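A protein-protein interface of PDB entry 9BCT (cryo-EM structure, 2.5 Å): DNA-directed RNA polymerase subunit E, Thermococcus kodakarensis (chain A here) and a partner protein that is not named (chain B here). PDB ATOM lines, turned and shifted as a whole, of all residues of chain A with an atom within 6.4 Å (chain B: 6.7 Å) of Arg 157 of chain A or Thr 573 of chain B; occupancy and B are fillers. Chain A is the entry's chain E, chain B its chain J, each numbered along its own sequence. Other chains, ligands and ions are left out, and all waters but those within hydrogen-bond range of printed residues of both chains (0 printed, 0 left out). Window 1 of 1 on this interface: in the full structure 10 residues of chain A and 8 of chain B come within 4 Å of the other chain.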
ATOM      1  N   GLY A  36     -35.488  12.073  24.253  1.00  0.00           N
ATOM      2  CA  GLY A  36     -34.239  11.352  24.383  1.00  0.00           C
ATOM      3  C   GLY A  36     -33.557  11.458  25.727  1.00  0.00           C
ATOM      4  O   GLY A  36     -32.397  11.050  25.845  1.00  0.00           O
ATOM      5  N   MET A 104     -35.541   1.076  27.082  1.00  0.00           N
ATOM      6  CA  MET A 104     -34.426   0.619  27.896  1.00  0.00           C
ATOM      7  C   MET A 104     -34.128  -0.853  27.628  1.00  0.00           C
ATOM      8  O   MET A 104     -34.882  -1.559  26.954  1.00  0.00           O
ATOM      9  CB  MET A 104     -34.726   0.841  29.381  1.00  0.00           C
ATOM     10  CG  MET A 104     -34.947   2.293  29.757  1.00  0.00           C
ATOM     11  SD  MET A 104     -34.060   2.735  31.261  1.00  0.00           S
ATOM     12  CE  MET A 104     -32.423   2.126  30.872  1.00  0.00           C
ATOM     13  N   ASP A 105     -33.003  -1.310  28.172  1.00  0.00           N
ATOM     14  CA  ASP A 105     -32.562  -2.696  28.050  1.00  0.00           C
ATOM     15  C   ASP A 105     -32.380  -3.262  29.452  1.00  0.00           C
ATOM     16  O   ASP A 105     -31.492  -2.827  30.192  1.00  0.00           O
ATOM     17  CB  ASP A 105     -31.267  -2.791  27.245  1.00  0.00           C
ATOM     18  CG  ASP A 105     -31.514  -2.938  25.756  1.00  0.00           C
ATOM     19  OD1 ASP A 105     -32.079  -2.004  25.150  1.00  0.00           O
ATOM     20  OD2 ASP A 105     -31.144  -3.989  25.192  1.00  0.00           O
ATOM     21  N   SER A 153     -28.637   8.952  36.847  1.00  0.00           N
ATOM     22  CA  SER A 153     -28.239   9.812  35.744  1.00  0.00           C
ATOM     23  C   SER A 153     -29.449  10.120  34.876  1.00  0.00           C
ATOM     24  O   SER A 153     -30.435   9.379  34.858  1.00  0.00           O
ATOM     25  CB  SER A 153     -27.133   9.167  34.896  1.00  0.00           C
ATOM     26  OG  SER A 153     -27.660   8.641  33.692  1.00  0.00           O
ATOM     27  N   VAL A 155     -29.230  10.239  31.624  1.00  0.00           N
ATOM     28  CA  VAL A 155     -29.012   9.574  30.345  1.00  0.00           C
ATOM     29  C   VAL A 155     -29.637   8.189  30.400  1.00  0.00           C
ATOM     30  O   VAL A 155     -29.489   7.461  31.388  1.00  0.00           O
ATOM     31  CB  VAL A 155     -27.510   9.498  30.014  1.00  0.00           C
ATOM     32  CG1 VAL A 155     -27.308   9.200  28.538  1.00  0.00           C
ATOM     33  CG2 VAL A 155     -26.816  10.793  30.403  1.00  0.00           C
ATOM     34  N   ILE A 156     -30.352   7.826  29.332  1.00  0.00           N
ATOM     35  CA  ILE A 156     -31.069   6.556  29.306  1.00  0.00           C
ATOM     36  C   ILE A 156     -30.097   5.381  29.319  1.00  0.00           C
ATOM     37  O   ILE A 156     -30.319   4.387  30.020  1.00  0.00           O
ATOM     38  CB  ILE A 156     -32.006   6.501  28.087  1.00  0.00           C
ATOM     39  CG1 ILE A 156     -32.651   7.867  27.853  1.00  0.00           C
ATOM     40  CG2 ILE A 156     -33.067   5.430  28.278  1.00  0.00           C
ATOM     41  CD1 ILE A 156     -33.431   7.962  26.562  1.00  0.00           C
ATOM     42  N   ARG A 157     -29.011   5.473  28.549  1.00  0.00           N
ATOM     43  CA  ARG A 157     -28.072   4.358  28.456  1.00  0.00           C
ATOM     44  C   ARG A 157     -27.361   4.109  29.782  1.00  0.00           C
ATOM     45  O   ARG A 157     -27.123   2.954  30.155  1.00  0.00           O
ATOM     46  CB  ARG A 157     -27.057   4.619  27.345  1.00  0.00           C
ATOM     47  CG  ARG A 157     -27.672   4.801  25.968  1.00  0.00           C
ATOM     48  CD  ARG A 157     -27.913   3.462  25.293  1.00  0.00           C
ATOM     49  NE  ARG A 157     -26.715   2.631  25.298  1.00  0.00           N
ATOM     50  CZ  ARG A 157     -26.674   1.370  24.891  1.00  0.00           C
ATOM     51  NH1 ARG A 157     -27.754   0.758  24.432  1.00  0.00           N
ATOM     52  NH2 ARG A 157     -25.523   0.707  24.946  1.00  0.00           N
ATOM     53  N   GLU A 158     -27.010   5.175  30.505  1.00  0.00           N
ATOM     54  CA  GLU A 158     -26.322   5.015  31.781  1.00  0.00           C
ATOM     55  C   GLU A 158     -27.219   4.422  32.860  1.00  0.00           C
ATOM     56  O   GLU A 158     -26.703   3.876  33.842  1.00  0.00           O
ATOM     57  CB  GLU A 158     -25.761   6.359  32.248  1.00  0.00           C
ATOM     58  CG  GLU A 158     -24.971   7.101  31.185  1.00  0.00           C
ATOM     59  CD  GLU A 158     -23.896   7.993  31.772  1.00  0.00           C
ATOM     60  OE1 GLU A 158     -24.186   8.711  32.752  1.00  0.00           O
ATOM     61  OE2 GLU A 158     -22.760   7.976  31.253  1.00  0.00           O
ATOM     62  N   ASN A 159     -28.536   4.520  32.708  1.00  0.00           N
ATOM     63  CA  ASN A 159     -29.446   3.921  33.675  1.00  0.00           C
ATOM     64  C   ASN A 159     -29.422   2.403  33.556  1.00  0.00           C
ATOM     65  O   ASN A 159     -29.310   1.849  32.458  1.00  0.00           O
ATOM     66  CB  ASN A 159     -30.864   4.448  33.465  1.00  0.00           C
ATOM     67  CG  ASN A 159     -31.032   5.873  33.951  1.00  0.00           C
ATOM     68  OD1 ASN A 159     -31.592   6.718  33.254  1.00  0.00           O
ATOM     69  ND2 ASN A 159     -30.542   6.148  35.153  1.00  0.00           N
ATOM     70  N   LYS A 160     -29.528   1.727  34.697  1.00  0.00           N
ATOM     71  CA  LYS A 160     -29.430   0.276  34.768  1.00  0.00           C
ATOM     72  C   LYS A 160     -30.748  -0.305  35.257  1.00  0.00           C
ATOM     73  O   LYS A 160     -31.325   0.186  36.234  1.00  0.00           O
ATOM     74  CB  LYS A 160     -28.287  -0.152  35.693  1.00  0.00           C
ATOM     75  CG  LYS A 160     -27.018   0.668  35.527  1.00  0.00           C
ATOM     76  CD  LYS A 160     -26.412   0.477  34.148  1.00  0.00           C
ATOM     77  CE  LYS A 160     -25.343  -0.602  34.160  1.00  0.00           C
ATOM     78  NZ  LYS A 160     -24.255  -0.307  33.188  1.00  0.00           N
ATOM     79  N   GLN B 556     -17.771  -5.333  20.170  1.00  0.00           N
ATOM     80  CA  GLN B 556     -19.075  -5.090  19.563  1.00  0.00           C
ATOM     81  C   GLN B 556     -18.954  -4.846  18.064  1.00  0.00           C
ATOM     82  O   GLN B 556     -19.756  -5.363  17.278  1.00  0.00           O
ATOM     83  CB  GLN B 556     -19.757  -3.905  20.244  1.00  0.00           C
ATOM     84  CG  GLN B 556     -20.366  -4.232  21.597  1.00  0.00           C
ATOM     85  CD  GLN B 556     -21.127  -3.062  22.189  1.00  0.00           C
ATOM     86  OE1 GLN B 556     -20.709  -2.476  23.187  1.00  0.00           O
ATOM     87  NE2 GLN B 556     -22.253  -2.719  21.575  1.00  0.00           N
ATOM     88  N   ILE B 564     -24.089   0.504  16.420  1.00  0.00           N
ATOM     89  CA  ILE B 564     -23.729   0.436  17.834  1.00  0.00           C
ATOM     90  C   ILE B 564     -24.248   1.697  18.516  1.00  0.00           C
ATOM     91  O   ILE B 564     -23.786   2.799  18.183  1.00  0.00           O
ATOM     92  CB  ILE B 564     -22.214   0.291  18.025  1.00  0.00           C
ATOM     93  CG1 ILE B 564     -21.750  -1.096  17.579  1.00  0.00           C
ATOM     94  CG2 ILE B 564     -21.840   0.519  19.479  1.00  0.00           C
ATOM     95  CD1 ILE B 564     -20.503  -1.074  16.725  1.00  0.00           C
ATOM     96  N   PRO B 565     -25.196   1.592  19.449  1.00  0.00           N
ATOM     97  CA  PRO B 565     -25.663   2.779  20.184  1.00  0.00           C
ATOM     98  C   PRO B 565     -24.700   3.128  21.310  1.00  0.00           C
ATOM     99  O   PRO B 565     -24.373   2.286  22.149  1.00  0.00           O
ATOM    100  CB  PRO B 565     -27.031   2.343  20.723  1.00  0.00           C
ATOM    101  CG  PRO B 565     -26.922   0.859  20.861  1.00  0.00           C
ATOM    102  CD  PRO B 565     -25.952   0.378  19.810  1.00  0.00           C
ATOM    103  N   ILE B 566     -24.237   4.378  21.323  1.00  0.00           N
ATOM    104  CA  ILE B 566     -23.301   4.861  22.328  1.00  0.00           C
ATOM    105  C   ILE B 566     -23.839   6.153  22.922  1.00  0.00           C
ATOM    106  O   ILE B 566     -24.742   6.788  22.369  1.00  0.00           O
ATOM    107  CB  ILE B 566     -21.884   5.086  21.753  1.00  0.00           C
ATOM    108  CG1 ILE B 566     -21.894   6.216  20.719  1.00  0.00           C
ATOM    109  CG2 ILE B 566     -21.326   3.799  21.160  1.00  0.00           C
ATOM    110  CD1 ILE B 566     -21.196   7.482  21.177  1.00  0.00           C
ATOM    111  N   VAL B 567     -23.273   6.541  24.064  1.00  0.00           N
ATOM    112  CA  VAL B 567     -23.644   7.801  24.697  1.00  0.00           C
ATOM    113  C   VAL B 567     -22.890   8.934  24.013  1.00  0.00           C
ATOM    114  O   VAL B 567     -21.674   9.080  24.179  1.00  0.00           O
ATOM    115  CB  VAL B 567     -23.348   7.770  26.201  1.00  0.00           C
ATOM    116  CG1 VAL B 567     -23.675   9.117  26.832  1.00  0.00           C
ATOM    117  CG2 VAL B 567     -24.125   6.657  26.873  1.00  0.00           C
ATOM    118  N   GLY B 568     -23.611   9.740  23.239  1.00  0.00           N
ATOM    119  CA  GLY B 568     -23.043  10.909  22.605  1.00  0.00           C
ATOM    120  C   GLY B 568     -23.102  12.122  23.512  1.00  0.00           C
ATOM    121  O   GLY B 568     -23.359  12.033  24.713  1.00  0.00           O
ATOM    122  N   GLU B 569     -22.852  13.283  22.913  1.00  0.00           N
ATOM    123  CA  GLU B 569     -22.965  14.529  23.649  1.00  0.00           C
ATOM    124  C   GLU B 569     -24.433  14.868  23.899  1.00  0.00           C
ATOM    125  O   GLU B 569     -25.346  14.266  23.325  1.00  0.00           O
ATOM    126  CB  GLU B 569     -22.274  15.666  22.896  1.00  0.00           C
ATOM    127  CG  GLU B 569     -20.904  15.301  22.348  1.00  0.00           C
ATOM    128  CD  GLU B 569     -20.009  14.665  23.395  1.00  0.00           C
ATOM    129  OE1 GLU B 569     -19.604  15.373  24.342  1.00  0.00           O
ATOM    130  OE2 GLU B 569     -19.709  13.459  23.272  1.00  0.00           O
ATOM    131  N   GLY B 571     -26.101  14.084  26.337  1.00  0.00           N
ATOM    132  CA  GLY B 571     -26.797  13.006  27.021  1.00  0.00           C
ATOM    133  C   GLY B 571     -27.848  12.311  26.187  1.00  0.00           C
ATOM    134  O   GLY B 571     -28.866  11.868  26.729  1.00  0.00           O
ATOM    135  N   ARG B 572     -27.631  12.201  24.880  1.00  0.00           N
ATOM    136  CA  ARG B 572     -28.561  11.538  23.980  1.00  0.00           C
ATOM    137  C   ARG B 572     -27.850  10.410  23.250  1.00  0.00           C
ATOM    138  O   ARG B 572     -26.679  10.538  22.878  1.00  0.00           O
ATOM    139  CB  ARG B 572     -29.162  12.523  22.971  1.00  0.00           C
ATOM    140  CG  ARG B 572     -29.429  13.907  23.537  1.00  0.00           C
ATOM    141  CD  ARG B 572     -30.791  13.967  24.211  1.00  0.00           C
ATOM    142  NE  ARG B 572     -31.109  15.308  24.685  1.00  0.00           N
ATOM    143  CZ  ARG B 572     -32.018  16.101  24.134  1.00  0.00           C
ATOM    144  NH1 ARG B 572     -32.720  15.721  23.079  1.00  0.00           N
ATOM    145  NH2 ARG B 572     -32.227  17.308  24.653  1.00  0.00           N
ATOM    146  N   THR B 573     -28.563   9.306  23.052  1.00  0.00           N
ATOM    147  CA  THR B 573     -27.979   8.143  22.400  1.00  0.00           C
ATOM    148  C   THR B 573     -27.782   8.413  20.915  1.00  0.00           C
ATOM    149  O   THR B 573     -28.744   8.688  20.191  1.00  0.00           O
ATOM    150  CB  THR B 573     -28.877   6.924  22.603  1.00  0.00           C
ATOM    151  OG1 THR B 573     -29.268   6.842  23.979  1.00  0.00           O
ATOM    152  CG2 THR B 573     -28.142   5.652  22.215  1.00  0.00           C
ATOM    153  N   GLU B 574     -26.534   8.337  20.464  1.00  0.00           N
ATOM    154  CA  GLU B 574     -26.192   8.468  19.056  1.00  0.00           C
ATOM    155  C   GLU B 574     -25.678   7.125  18.553  1.00  0.00           C
ATOM    156  O   GLU B 574     -24.922   6.439  19.252  1.00  0.00           O
ATOM    157  CB  GLU B 574     -25.169   9.592  18.836  1.00  0.00           C
ATOM    158  CG  GLU B 574     -23.699   9.187  18.874  1.00  0.00           C
ATOM    159  CD  GLU B 574     -22.796  10.161  18.143  1.00  0.00           C
ATOM    160  OE1 GLU B 574     -21.561  10.001  18.230  1.00  0.00           O
ATOM    161  OE2 GLU B 574     -23.316  11.082  17.480  1.00  0.00           O
ATOM    162  N   VAL B 575     -26.145   6.721  17.378  1.00  0.00           N
ATOM    163  CA  VAL B 575     -25.793   5.435  16.792  1.00  0.00           C
ATOM    164  C   VAL B 575     -24.606   5.624  15.860  1.00  0.00           C
ATOM    165  O   VAL B 575     -24.492   6.650  15.178  1.00  0.00           O
ATOM    166  CB  VAL B 575     -26.990   4.808  16.054  1.00  0.00           C
ATOM    167  CG1 VAL B 575     -28.110   4.517  17.030  1.00  0.00           C
ATOM    168  CG2 VAL B 575     -27.490   5.728  14.949  1.00  0.00           C
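The backbone NH (N) of Val 155 of chain A lies within hydrogen-bond range of the side-chain hydroxyl (OG) of Ser 153 of chain A (3.0 Å).
O of Val 155 of chain A sits close to OD1 of Asn 159 of chain A (2.9 Å).
Among the printed residues, merely in contact across the chains: Gly 36 of chain A with Gly 571 of chain B (3.7 Å), Gly 36 of chain A with Arg 572 of chain B (3.7 Å), Val 155 of chain A with Gly 571 of chain B (3.6 Å), Arg 157 of chain A with Val 567 of chain B (3.6 Å) and Arg 157 of chain A with Thr 573 of chain B (3.3 Å).
Of the 12 printed residues of chain B, 5 touch a printed residue of chain A.
Hydrophobic or aromatic side chains of chain B within 4 Å of the printed part of chain A: Pro 565 and Val 567.
Hydrophobic or aromatic side chains of chain A that line the printed part of chain B: Val 155.
Among the printed residues, 6 pairs touch across the chains.
Printed residues of chain B within 4 Å of Val 155 of chain A: Gly 571 (3.6 Å).
Of chain B, only Pro 565 (3.4 Å), Val 567 (3.6 Å) and Thr 573 (3.3 Å) come within 4 Å of Arg 157 of chain A.
Printed residues of chain A within 4 Å of Pro 565 of chain B: Arg 157.
Of the printed residues of chain A, Val 567 of chain B touches Arg 157 (3.6 Å).
Glu 569 of chain B touches none of the printed residues of chain A.
Of the printed residues of chain A, Arg 572 of chain B touches Gly 36 (3.7 Å).
Thr 573 of chain B touches just one residue of chain A: Arg 157 (3.3 Å).
The nearest residue of chain B that does not touch Arg 157 of chain A is Ile 566 of chain B (5.0 Å).
The nearest residue of chain A that does not touch Thr 573 of chain B is Ile 156 of chain A (4.9 Å).
The guanidinium group of Arg 157 of chain A lies within hydrogen-bond range of the backbone carbonyl oxygen of Pro 565 of chain B, at 3.4 Å.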
